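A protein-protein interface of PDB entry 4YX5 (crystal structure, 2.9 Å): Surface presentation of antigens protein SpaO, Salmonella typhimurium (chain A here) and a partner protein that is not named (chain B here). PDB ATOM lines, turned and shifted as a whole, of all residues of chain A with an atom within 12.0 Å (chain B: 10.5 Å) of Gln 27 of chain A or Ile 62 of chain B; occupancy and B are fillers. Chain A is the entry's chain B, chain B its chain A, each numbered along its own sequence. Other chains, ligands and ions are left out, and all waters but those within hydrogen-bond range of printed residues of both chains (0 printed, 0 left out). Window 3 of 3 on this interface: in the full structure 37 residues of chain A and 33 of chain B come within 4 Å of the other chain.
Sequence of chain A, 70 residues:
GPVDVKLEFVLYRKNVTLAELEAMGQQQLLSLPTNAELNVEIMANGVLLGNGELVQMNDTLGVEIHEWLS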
ATOM      1  N   LEU A  11     -23.266  17.103   7.342  1.00  0.00           N
ATOM      2  CA  LEU A  11     -22.017  17.856   7.260  1.00  0.00           C
ATOM      3  C   LEU A  11     -21.044  17.263   6.243  1.00  0.00           C
ATOM      4  O   LEU A  11     -20.437  17.983   5.448  1.00  0.00           O
ATOM      5  CB  LEU A  11     -21.359  17.901   8.629  1.00  0.00           C
ATOM      6  CG  LEU A  11     -20.073  18.701   8.639  1.00  0.00           C
ATOM      7  CD1 LEU A  11     -20.370  20.106   8.135  1.00  0.00           C
ATOM      8  CD2 LEU A  11     -19.458  18.714  10.031  1.00  0.00           C
ATOM      9  N   TYR A  12     -20.917  15.938   6.256  1.00  0.00           N
ATOM     10  CA  TYR A  12     -19.977  15.244   5.379  1.00  0.00           C
ATOM     11  C   TYR A  12     -20.451  13.822   5.115  1.00  0.00           C
ATOM     12  O   TYR A  12     -21.020  13.171   5.996  1.00  0.00           O
ATOM     13  CB  TYR A  12     -18.566  15.258   6.005  1.00  0.00           C
ATOM     14  CG  TYR A  12     -17.405  14.794   5.131  1.00  0.00           C
ATOM     15  CD1 TYR A  12     -17.015  15.502   4.001  1.00  0.00           C
ATOM     16  CD2 TYR A  12     -16.663  13.676   5.483  1.00  0.00           C
ATOM     17  CE1 TYR A  12     -15.941  15.078   3.233  1.00  0.00           C
ATOM     18  CE2 TYR A  12     -15.604  13.245   4.720  1.00  0.00           C
ATOM     19  CZ  TYR A  12     -15.238  13.942   3.600  1.00  0.00           C
ATOM     20  OH  TYR A  12     -14.166  13.485   2.851  1.00  0.00           O
ATOM     21  N   ALA A  19     -10.974  -1.260   5.763  1.00  0.00           N
ATOM     22  CA  ALA A  19      -9.778  -0.749   6.405  1.00  0.00           C
ATOM     23  C   ALA A  19     -10.094   0.544   7.146  1.00  0.00           C
ATOM     24  O   ALA A  19     -10.102   0.567   8.370  1.00  0.00           O
ATOM     25  CB  ALA A  19      -8.681  -0.527   5.385  1.00  0.00           C
ATOM     26  N   GLU A  20     -10.384   1.607   6.402  1.00  0.00           N
ATOM     27  CA  GLU A  20     -10.640   2.932   6.971  1.00  0.00           C
ATOM     28  C   GLU A  20     -11.730   2.907   8.050  1.00  0.00           C
ATOM     29  O   GLU A  20     -11.804   3.780   8.910  1.00  0.00           O
ATOM     30  CB  GLU A  20     -11.039   3.897   5.862  1.00  0.00           C
ATOM     31  CG  GLU A  20     -10.010   4.077   4.764  1.00  0.00           C
ATOM     32  CD  GLU A  20     -10.635   4.482   3.427  1.00  0.00           C
ATOM     33  OE1 GLU A  20     -11.804   4.112   3.164  1.00  0.00           O
ATOM     34  OE2 GLU A  20      -9.955   5.178   2.639  1.00  0.00           O
ATOM     35  N   LEU A  21     -12.581   1.895   7.993  1.00  0.00           N
ATOM     36  CA  LEU A  21     -13.581   1.673   9.027  1.00  0.00           C
ATOM     37  C   LEU A  21     -12.943   1.242  10.345  1.00  0.00           C
ATOM     38  O   LEU A  21     -13.256   1.793  11.398  1.00  0.00           O
ATOM     39  CB  LEU A  21     -14.571   0.620   8.565  1.00  0.00           C
ATOM     40  CG  LEU A  21     -15.973   0.817   9.095  1.00  0.00           C
ATOM     41  CD1 LEU A  21     -16.352   2.277   8.992  1.00  0.00           C
ATOM     42  CD2 LEU A  21     -16.932  -0.030   8.285  1.00  0.00           C
ATOM     43  N   GLU A  22     -12.060   0.248  10.278  1.00  0.00           N
ATOM     44  CA  GLU A  22     -11.261  -0.155  11.428  1.00  0.00           C
ATOM     45  C   GLU A  22     -10.545   1.059  12.036  1.00  0.00           C
ATOM     46  O   GLU A  22     -10.631   1.300  13.237  1.00  0.00           O
ATOM     47  CB  GLU A  22     -10.245  -1.235  11.029  1.00  0.00           C
ATOM     48  N   ALA A  23      -9.876   1.841  11.193  1.00  0.00           N
ATOM     49  CA  ALA A  23      -9.059   2.971  11.640  1.00  0.00           C
ATOM     50  C   ALA A  23      -9.854   4.052  12.364  1.00  0.00           C
ATOM     51  O   ALA A  23      -9.301   4.846  13.127  1.00  0.00           O
ATOM     52  CB  ALA A  23      -8.322   3.583  10.456  1.00  0.00           C
ATOM     53  N   MET A  24     -11.154   4.095  12.124  1.00  0.00           N
ATOM     54  CA  MET A  24     -11.978   5.064  12.813  1.00  0.00           C
ATOM     55  C   MET A  24     -12.530   4.512  14.131  1.00  0.00           C
ATOM     56  O   MET A  24     -12.816   5.277  15.055  1.00  0.00           O
ATOM     57  CB  MET A  24     -13.108   5.517  11.907  1.00  0.00           C
ATOM     58  CG  MET A  24     -12.723   6.635  10.961  1.00  0.00           C
ATOM     59  SD  MET A  24     -14.200   7.201  10.086  1.00  0.00           S
ATOM     60  CE  MET A  24     -14.713   5.665   9.329  1.00  0.00           C
ATOM     61  N   GLY A  25     -12.667   3.187  14.214  1.00  0.00           N
ATOM     62  CA  GLY A  25     -13.088   2.515  15.440  1.00  0.00           C
ATOM     63  C   GLY A  25     -12.151   2.814  16.596  1.00  0.00           C
ATOM     64  O   GLY A  25     -12.517   2.695  17.769  1.00  0.00           O
ATOM     65  N   GLN A  26     -10.927   3.193  16.238  1.00  0.00           N
ATOM     66  CA  GLN A  26      -9.941   3.715  17.167  1.00  0.00           C
ATOM     67  C   GLN A  26     -10.369   5.104  17.605  1.00  0.00           C
ATOM     68  O   GLN A  26     -11.216   5.285  18.506  1.00  0.00           O
ATOM     69  CB  GLN A  26      -8.549   3.788  16.511  1.00  0.00           C
ATOM     70  CG  GLN A  26      -7.771   2.463  16.389  1.00  0.00           C
ATOM     71  CD  GLN A  26      -8.253   1.372  17.341  1.00  0.00           C
ATOM     72  OE1 GLN A  26      -9.140   0.585  17.000  1.00  0.00           O
ATOM     73  NE2 GLN A  26      -7.651   1.308  18.535  1.00  0.00           N
ATOM     74  N   GLN A  27      -9.763   6.077  16.934  1.00  0.00           N
ATOM     75  CA  GLN A  27     -10.078   7.477  17.101  1.00  0.00           C
ATOM     76  C   GLN A  27      -9.219   8.255  16.131  1.00  0.00           C
ATOM     77  O   GLN A  27      -8.760   9.346  16.443  1.00  0.00           O
ATOM     78  CB  GLN A  27      -9.834   7.943  18.540  1.00  0.00           C
ATOM     79  N   GLN A  28      -8.976   7.689  14.952  1.00  0.00           N
ATOM     80  CA  GLN A  28      -8.104   8.355  13.990  1.00  0.00           C
ATOM     81  C   GLN A  28      -8.890   9.437  13.264  1.00  0.00           C
ATOM     82  O   GLN A  28     -10.066   9.271  12.944  1.00  0.00           O
ATOM     83  CB  GLN A  28      -7.491   7.346  13.015  1.00  0.00           C
ATOM     84  CG  GLN A  28      -6.967   7.935  11.711  1.00  0.00           C
ATOM     85  CD  GLN A  28      -5.888   7.071  11.070  1.00  0.00           C
ATOM     86  OE1 GLN A  28      -4.794   6.918  11.620  1.00  0.00           O
ATOM     87  NE2 GLN A  28      -6.193   6.499   9.910  1.00  0.00           N
ATOM     88  N   LEU A  29      -8.223  10.557  13.029  1.00  0.00           N
ATOM     89  CA  LEU A  29      -8.855  11.749  12.497  1.00  0.00           C
ATOM     90  C   LEU A  29      -9.226  11.619  11.037  1.00  0.00           C
ATOM     91  O   LEU A  29      -8.412  11.193  10.221  1.00  0.00           O
ATOM     92  CB  LEU A  29      -7.927  12.955  12.689  1.00  0.00           C
ATOM     93  CG  LEU A  29      -8.361  14.346  12.203  1.00  0.00           C
ATOM     94  CD1 LEU A  29      -7.871  15.429  13.160  1.00  0.00           C
ATOM     95  CD2 LEU A  29      -7.851  14.637  10.789  1.00  0.00           C
ATOM     96  N   LEU A  30     -10.461  12.006  10.717  1.00  0.00           N
ATOM     97  CA  LEU A  30     -10.920  12.127   9.335  1.00  0.00           C
ATOM     98  C   LEU A  30     -10.829  13.588   8.881  1.00  0.00           C
ATOM     99  O   LEU A  30     -11.268  14.503   9.579  1.00  0.00           O
ATOM    100  CB  LEU A  30     -12.346  11.589   9.191  1.00  0.00           C
ATOM    101  CG  LEU A  30     -13.043  11.831   7.842  1.00  0.00           C
ATOM    102  CD1 LEU A  30     -12.341  11.144   6.667  1.00  0.00           C
ATOM    103  CD2 LEU A  30     -14.513  11.417   7.921  1.00  0.00           C
ATOM    104  N   SER A  31     -10.249  13.807   7.711  1.00  0.00           N
ATOM    105  CA  SER A  31      -9.853  15.148   7.331  1.00  0.00           C
ATOM    106  C   SER A  31     -10.898  15.834   6.477  1.00  0.00           C
ATOM    107  O   SER A  31     -11.067  15.527   5.299  1.00  0.00           O
ATOM    108  CB  SER A  31      -8.512  15.122   6.598  1.00  0.00           C
ATOM    109  OG  SER A  31      -7.952  16.428   6.519  1.00  0.00           O
ATOM    110  N   LEU A  32     -11.594  16.775   7.093  1.00  0.00           N
ATOM    111  CA  LEU A  32     -12.570  17.579   6.397  1.00  0.00           C
ATOM    112  C   LEU A  32     -11.881  18.828   5.944  1.00  0.00           C
ATOM    113  O   LEU A  32     -10.991  19.310   6.638  1.00  0.00           O
ATOM    114  CB  LEU A  32     -13.746  17.931   7.305  1.00  0.00           C
ATOM    115  CG  LEU A  32     -14.905  16.953   7.508  1.00  0.00           C
ATOM    116  CD1 LEU A  32     -14.459  15.492   7.613  1.00  0.00           C
ATOM    117  CD2 LEU A  32     -15.684  17.379   8.744  1.00  0.00           C
ATOM    118  N   PRO A  33     -12.302  19.378   4.797  1.00  0.00           N
ATOM    119  CA  PRO A  33     -11.743  20.674   4.413  1.00  0.00           C
ATOM    120  C   PRO A  33     -12.020  21.720   5.490  1.00  0.00           C
ATOM    121  O   PRO A  33     -12.800  21.473   6.414  1.00  0.00           O
ATOM    122  CB  PRO A  33     -12.471  21.008   3.107  1.00  0.00           C
ATOM    123  CG  PRO A  33     -13.674  20.113   3.073  1.00  0.00           C
ATOM    124  CD  PRO A  33     -13.317  18.889   3.847  1.00  0.00           C
ATOM    125  N   ALA A  36     -16.090  23.015   5.187  1.00  0.00           N
ATOM    126  CA  ALA A  36     -17.149  22.002   5.208  1.00  0.00           C
ATOM    127  C   ALA A  36     -18.513  22.601   5.519  1.00  0.00           C
ATOM    128  O   ALA A  36     -19.525  22.240   4.899  1.00  0.00           O
ATOM    129  CB  ALA A  36     -16.819  20.919   6.216  1.00  0.00           C
ATOM    130  N   GLU A  37     -18.524  23.525   6.476  1.00  0.00           N
ATOM    131  CA  GLU A  37     -19.750  24.161   6.931  1.00  0.00           C
ATOM    132  C   GLU A  37     -20.433  25.025   5.872  1.00  0.00           C
ATOM    133  O   GLU A  37     -21.502  25.559   6.110  1.00  0.00           O
ATOM    134  CB  GLU A  37     -19.466  25.005   8.165  1.00  0.00           C
ATOM    135  CG  GLU A  37     -19.418  24.214   9.445  1.00  0.00           C
ATOM    136  CD  GLU A  37     -18.105  23.477   9.665  1.00  0.00           C
ATOM    137  OE1 GLU A  37     -17.137  23.709   8.894  1.00  0.00           O
ATOM    138  OE2 GLU A  37     -18.051  22.668  10.627  1.00  0.00           O
ATOM    139  N   PHE B  14     -22.154  11.976   8.097  1.00  0.00           N
ATOM    140  CA  PHE B  14     -21.960  12.682   9.357  1.00  0.00           C
ATOM    141  C   PHE B  14     -23.059  13.719   9.579  1.00  0.00           C
ATOM    142  O   PHE B  14     -23.049  14.827   9.039  1.00  0.00           O
ATOM    143  CB  PHE B  14     -20.578  13.279   9.385  1.00  0.00           C
ATOM    144  CG  PHE B  14     -19.524  12.240   9.342  1.00  0.00           C
ATOM    145  CD1 PHE B  14     -18.992  11.738  10.504  1.00  0.00           C
ATOM    146  CD2 PHE B  14     -19.125  11.705   8.137  1.00  0.00           C
ATOM    147  CE1 PHE B  14     -18.057  10.754  10.465  1.00  0.00           C
ATOM    148  CE2 PHE B  14     -18.187  10.726   8.089  1.00  0.00           C
ATOM    149  CZ  PHE B  14     -17.647  10.247   9.257  1.00  0.00           C
ATOM    150  N   ALA B  42     -24.813  14.796  16.648  1.00  0.00           N
ATOM    151  CA  ALA B  42     -23.508  14.613  15.989  1.00  0.00           C
ATOM    152  C   ALA B  42     -23.257  13.123  15.813  1.00  0.00           C
ATOM    153  O   ALA B  42     -22.325  12.573  16.382  1.00  0.00           O
ATOM    154  CB  ALA B  42     -22.392  15.244  16.776  1.00  0.00           C
ATOM    155  N   GLU B  43     -24.111  12.467  15.042  1.00  0.00           N
ATOM    156  CA  GLU B  43     -24.034  11.031  14.905  1.00  0.00           C
ATOM    157  C   GLU B  43     -23.490  10.639  13.544  1.00  0.00           C
ATOM    158  O   GLU B  43     -23.471  11.431  12.600  1.00  0.00           O
ATOM    159  CB  GLU B  43     -25.406  10.397  15.151  1.00  0.00           C
ATOM    160  CG  GLU B  43     -25.792  10.393  16.634  1.00  0.00           C
ATOM    161  CD  GLU B  43     -27.272  10.722  16.908  1.00  0.00           C
ATOM    162  OE1 GLU B  43     -27.965  11.232  15.995  1.00  0.00           O
ATOM    163  OE2 GLU B  43     -27.739  10.473  18.053  1.00  0.00           O
ATOM    164  N   VAL B  44     -23.009   9.409  13.471  1.00  0.00           N
ATOM    165  CA  VAL B  44     -22.565   8.830  12.225  1.00  0.00           C
ATOM    166  C   VAL B  44     -23.555   7.774  11.800  1.00  0.00           C
ATOM    167  O   VAL B  44     -23.943   6.926  12.592  1.00  0.00           O
ATOM    168  CB  VAL B  44     -21.186   8.213  12.359  1.00  0.00           C
ATOM    169  CG1 VAL B  44     -20.661   7.812  11.004  1.00  0.00           C
ATOM    170  CG2 VAL B  44     -20.248   9.207  12.986  1.00  0.00           C
ATOM    171  N   GLY B  52     -22.638   5.749  16.055  1.00  0.00           N
ATOM    172  CA  GLY B  52     -22.063   6.416  17.196  1.00  0.00           C
ATOM    173  C   GLY B  52     -21.864   7.890  16.991  1.00  0.00           C
ATOM    174  O   GLY B  52     -22.164   8.417  15.934  1.00  0.00           O
ATOM    175  N   HIS B  53     -21.341   8.563  17.999  1.00  0.00           N
ATOM    176  CA  HIS B  53     -21.262  10.004  17.934  1.00  0.00           C
ATOM    177  C   HIS B  53     -19.880  10.447  17.507  1.00  0.00           C
ATOM    178  O   HIS B  53     -18.958   9.645  17.434  1.00  0.00           O
ATOM    179  CB  HIS B  53     -21.653  10.604  19.280  1.00  0.00           C
ATOM    180  CG  HIS B  53     -22.948  10.073  19.808  1.00  0.00           C
ATOM    181  ND1 HIS B  53     -23.075   8.810  20.344  1.00  0.00           N
ATOM    182  CD2 HIS B  53     -24.189  10.626  19.857  1.00  0.00           C
ATOM    183  CE1 HIS B  53     -24.324   8.613  20.721  1.00  0.00           C
ATOM    184  NE2 HIS B  53     -25.020   9.696  20.432  1.00  0.00           N
ATOM    185  N   PHE B  54     -19.746  11.730  17.205  1.00  0.00           N
ATOM    186  CA  PHE B  54     -18.495  12.264  16.703  1.00  0.00           C
ATOM    187  C   PHE B  54     -18.288  13.701  17.143  1.00  0.00           C
ATOM    188  O   PHE B  54     -19.224  14.433  17.370  1.00  0.00           O
ATOM    189  CB  PHE B  54     -18.417  12.160  15.164  1.00  0.00           C
ATOM    190  CG  PHE B  54     -19.292  13.149  14.403  1.00  0.00           C
ATOM    191  CD1 PHE B  54     -18.817  14.405  14.065  1.00  0.00           C
ATOM    192  CD2 PHE B  54     -20.559  12.796  13.968  1.00  0.00           C
ATOM    193  CE1 PHE B  54     -19.607  15.301  13.355  1.00  0.00           C
ATOM    194  CE2 PHE B  54     -21.348  13.687  13.263  1.00  0.00           C
ATOM    195  CZ  PHE B  54     -20.872  14.939  12.955  1.00  0.00           C
ATOM    196  N   ASN B  55     -17.036  14.095  17.248  1.00  0.00           N
ATOM    197  CA  ASN B  55     -16.690  15.432  17.648  1.00  0.00           C
ATOM    198  C   ASN B  55     -15.943  16.111  16.530  1.00  0.00           C
ATOM    199  O   ASN B  55     -15.054  15.509  15.919  1.00  0.00           O
ATOM    200  CB  ASN B  55     -15.860  15.397  18.931  1.00  0.00           C
ATOM    201  CG  ASN B  55     -16.723  15.234  20.167  1.00  0.00           C
ATOM    202  OD1 ASN B  55     -16.853  16.167  20.961  1.00  0.00           O
ATOM    203  ND2 ASN B  55     -17.345  14.060  20.323  1.00  0.00           N
ATOM    204  N   ARG B  56     -16.315  17.352  16.233  1.00  0.00           N
ATOM    205  CA  ARG B  56     -15.596  18.096  15.212  1.00  0.00           C
ATOM    206  C   ARG B  56     -14.430  18.801  15.862  1.00  0.00           C
ATOM    207  O   ARG B  56     -14.548  19.368  16.940  1.00  0.00           O
ATOM    208  CB  ARG B  56     -16.481  19.102  14.484  1.00  0.00           C
ATOM    209  CG  ARG B  56     -15.925  19.483  13.123  1.00  0.00           C
ATOM    210  CD  ARG B  56     -16.485  20.791  12.615  1.00  0.00           C
ATOM    211  NE  ARG B  56     -16.170  21.093  11.210  1.00  0.00           N
ATOM    212  CZ  ARG B  56     -14.955  21.142  10.666  1.00  0.00           C
ATOM    213  NH1 ARG B  56     -13.855  20.934  11.381  1.00  0.00           N
ATOM    214  NH2 ARG B  56     -14.844  21.438   9.386  1.00  0.00           N
ATOM    215  N   VAL B  57     -13.288  18.725  15.201  1.00  0.00           N
ATOM    216  CA  VAL B  57     -12.039  19.240  15.725  1.00  0.00           C
ATOM    217  C   VAL B  57     -11.395  19.999  14.576  1.00  0.00           C
ATOM    218  O   VAL B  57     -11.983  20.072  13.491  1.00  0.00           O
ATOM    219  CB  VAL B  57     -11.140  18.106  16.261  1.00  0.00           C
ATOM    220  CG1 VAL B  57     -11.850  17.367  17.404  1.00  0.00           C
ATOM    221  CG2 VAL B  57     -10.791  17.127  15.143  1.00  0.00           C
ATOM    222  N   GLU B  58     -10.211  20.567  14.793  1.00  0.00           N
ATOM    223  CA  GLU B  58      -9.680  21.535  13.833  1.00  0.00           C
ATOM    224  C   GLU B  58      -9.323  20.876  12.504  1.00  0.00           C
ATOM    225  O   GLU B  58      -9.357  21.530  11.455  1.00  0.00           O
ATOM    226  CB  GLU B  58      -8.465  22.275  14.405  1.00  0.00           C
ATOM    227  CG  GLU B  58      -8.080  23.537  13.613  1.00  0.00           C
ATOM    228  CD  GLU B  58      -7.497  24.646  14.483  1.00  0.00           C
ATOM    229  OE1 GLU B  58      -6.251  24.769  14.567  1.00  0.00           O
ATOM    230  OE2 GLU B  58      -8.297  25.393  15.086  1.00  0.00           O
ATOM    231  N   GLY B  59      -9.004  19.584  12.539  1.00  0.00           N
ATOM    232  CA  GLY B  59      -8.687  18.852  11.319  1.00  0.00           C
ATOM    233  C   GLY B  59      -9.926  18.391  10.573  1.00  0.00           C
ATOM    234  O   GLY B  59     -10.023  18.481   9.345  1.00  0.00           O
ATOM    235  N   GLY B  60     -10.887  17.897  11.338  1.00  0.00           N
ATOM    236  CA  GLY B  60     -12.130  17.417  10.788  1.00  0.00           C
ATOM    237  C   GLY B  60     -12.887  16.710  11.883  1.00  0.00           C
ATOM    238  O   GLY B  60     -13.455  17.349  12.770  1.00  0.00           O
ATOM    239  N   ILE B  61     -12.874  15.385  11.849  1.00  0.00           N
ATOM    240  CA  ILE B  61     -13.733  14.653  12.751  1.00  0.00           C
ATOM    241  C   ILE B  61     -12.994  13.564  13.499  1.00  0.00           C
ATOM    242  O   ILE B  61     -12.145  12.896  12.933  1.00  0.00           O
ATOM    243  CB  ILE B  61     -14.912  14.039  11.981  1.00  0.00           C
ATOM    244  CG1 ILE B  61     -15.802  15.154  11.442  1.00  0.00           C
ATOM    245  CG2 ILE B  61     -15.731  13.109  12.870  1.00  0.00           C
ATOM    246  CD1 ILE B  61     -16.955  14.662  10.632  1.00  0.00           C
ATOM    247  N   ILE B  62     -13.315  13.408  14.779  1.00  0.00           N
ATOM    248  CA  ILE B  62     -12.870  12.258  15.554  1.00  0.00           C
ATOM    249  C   ILE B  62     -14.106  11.534  16.069  1.00  0.00           C
ATOM    250  O   ILE B  62     -15.041  12.169  16.547  1.00  0.00           O
ATOM    251  CB  ILE B  62     -11.970  12.668  16.738  1.00  0.00           C
ATOM    252  CG1 ILE B  62     -10.732  13.406  16.227  1.00  0.00           C
ATOM    253  CG2 ILE B  62     -11.590  11.451  17.575  1.00  0.00           C
ATOM    254  CD1 ILE B  62     -10.021  14.206  17.287  1.00  0.00           C
ATOM    255  N   VAL B  63     -14.106  10.210  15.975  1.00  0.00           N
ATOM    256  CA  VAL B  63     -15.297   9.443  16.266  1.00  0.00           C
ATOM    257  C   VAL B  63     -15.151   8.642  17.549  1.00  0.00           C
ATOM    258  O   VAL B  63     -14.188   7.908  17.721  1.00  0.00           O
ATOM    259  CB  VAL B  63     -15.627   8.488  15.101  1.00  0.00           C
ATOM    260  CG1 VAL B  63     -16.892   7.695  15.400  1.00  0.00           C
ATOM    261  CG2 VAL B  63     -15.766   9.266  13.785  1.00  0.00           C
ATOM    262  N   GLU B  64     -16.111   8.776  18.454  1.00  0.00           N
ATOM    263  CA  GLU B  64     -16.117   7.938  19.645  1.00  0.00           C
ATOM    264  C   GLU B  64     -16.503   6.502  19.270  1.00  0.00           C
ATOM    265  O   GLU B  64     -16.908   6.247  18.135  1.00  0.00           O
ATOM    266  CB  GLU B  64     -17.066   8.520  20.703  1.00  0.00           C
ATOM    267  CG  GLU B  64     -18.431   7.836  20.865  1.00  0.00           C
ATOM    268  CD  GLU B  64     -19.279   8.520  21.937  1.00  0.00           C
ATOM    269  OE1 GLU B  64     -18.742   9.436  22.609  1.00  0.00           O
ATOM    270  OE2 GLU B  64     -20.465   8.146  22.113  1.00  0.00           O
ATOM    271  N   THR B  65     -16.350   5.582  20.221  1.00  0.00           N
ATOM    272  CA  THR B  65     -16.682   4.168  20.041  1.00  0.00           C
ATOM    273  C   THR B  65     -17.782   3.934  19.000  1.00  0.00           C
ATOM    274  O   THR B  65     -18.926   4.349  19.193  1.00  0.00           O
ATOM    275  CB  THR B  65     -17.117   3.530  21.384  1.00  0.00           C
ATOM    276  N   LEU B  66     -17.405   3.307  17.884  1.00  0.00           N
ATOM    277  CA  LEU B  66     -18.307   3.093  16.749  1.00  0.00           C
ATOM    278  C   LEU B  66     -18.744   1.634  16.590  1.00  0.00           C
ATOM    279  O   LEU B  66     -17.913   0.747  16.405  1.00  0.00           O
ATOM    280  CB  LEU B  66     -17.636   3.568  15.460  1.00  0.00           C
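The backbone carbonyl oxygen of Gly 59 of chain B lies within hydrogen-bond range of the backbone NH of Leu 32 of chain A (3.2 Å).
The backbone carbonyl oxygen (O) of Phe 14 of chain B is in hydrogen-bond range of the backbone NH (N) of Leu 11 of chain A (2.8 Å).
N of Phe 14 of chain B is in hydrogen-bond range of O of Tyr 12 of chain A (2.7 Å).
NE of Arg 56 of chain B is in salt-bridge range of OE2 of Glu 37 of chain A (2.5 Å).
O of Leu 30 of chain A is in hydrogen-bond range of N of Ile 61 of chain B (2.9 Å).
The backbone NH (N) of Asn 55 of chain B is in hydrogen-bond range of the backbone carbonyl oxygen (O) of Ile 62 of chain B, at 2.9 Å.
Among the printed residues, pairs that only touch across the chains: Met 24 of chain A with Val 63 of chain B, Gln 27 of chain A with Ile 62 of chain B, Leu 29 of chain A with Val 57 of chain B, Leu 29 of chain A with Gly 59 of chain B, Leu 29 of chain A with Ile 61 of chain B, Leu 30 of chain A with Phe 14 of chain B, Leu 30 of chain A with Gly 60 of chain B, Ser 31 of chain A with Gly 59 of chain B, Leu 32 of chain A with Gly 60 of chain B, Leu 32 of chain A with Ile 61 of chain B, Pro 33 of chain A with Arg 56 of chain B and Ala 36 of chain A with Arg 56 of chain B.
Gln 27 of chain A touches just one residue of chain B: Ile 62.
No residue of chain B comes within 4 Å of Gly 25 of chain A.
No residue of chain B comes within 4 Å of Gln 26 of chain A.
No residue of chain A comes within 4 Å of Phe 54 of chain B.
Asn 55 of chain B touches none of the printed residues of chain A.
Val 57 of chain B touches one residue of chain A.
Ile 61 of chain B touches just these residues of chain A: Leu 29 (3.5 Å), Leu 30 (2.9 Å) and Leu 32 (3.5 Å).
Printed residues of chain B within 4 Å of Glu 37 of chain A: Arg 56.
Printed residues of chain B within 4 Å of Ser 31 of chain A: Gly 59 (3.9 Å).
Of the printed residues of chain A, Arg 56 of chain B touches Pro 33 (3.6 Å), Ala 36 (3.8 Å) and Glu 37 (2.5 Å).
Printed residues of chain B within 4 Å of Met 24 of chain A: Val 63.
Of the printed residues of chain A, Val 63 of chain B touches Met 24 (3.99 Å).
The nearest residue of chain B that does not touch Gln 27 of chain A is Val 63 of chain B (4.2 Å).
The nearest residue of chain A that does not touch Ile 62 of chain B is Leu 29 of chain A (4.5 Å).
Printed residues of chain A that touch a printed residue of chain B: Leu 11, Tyr 12, Met 24, Gln 27, Leu 29, Leu 30, Ser 31, Leu 32, Pro 33, Ala 36 and Glu 37.
Hydrophobic or aromatic side chains of chain A that line the printed part of chain B: Leu 11, Leu 29, Leu 30, Leu 32 and Ala 36.
Along chain A the printed residues that touch a printed residue of chain B span positions 11 to 37.
Printed residues of chain B that touch a printed residue of chain A: Phe 14, Arg 56, Val 57, Gly 59, Gly 60, Ile 61, Ile 62 and Val 63.
Hydrophobic or aromatic side chains of chain B that line the printed part of chain A: Phe 14, Val 57, Ile 61 and Ile 62.
Among the printed residues, 17 pairs touch across the chains.
Among the printed residues, Asp or Glu carboxylates within 4 Å of a Lys or Arg side-chain nitrogen of the other chain: Glu 37 of chain A with Arg 56 of chain B (2.5 Å).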
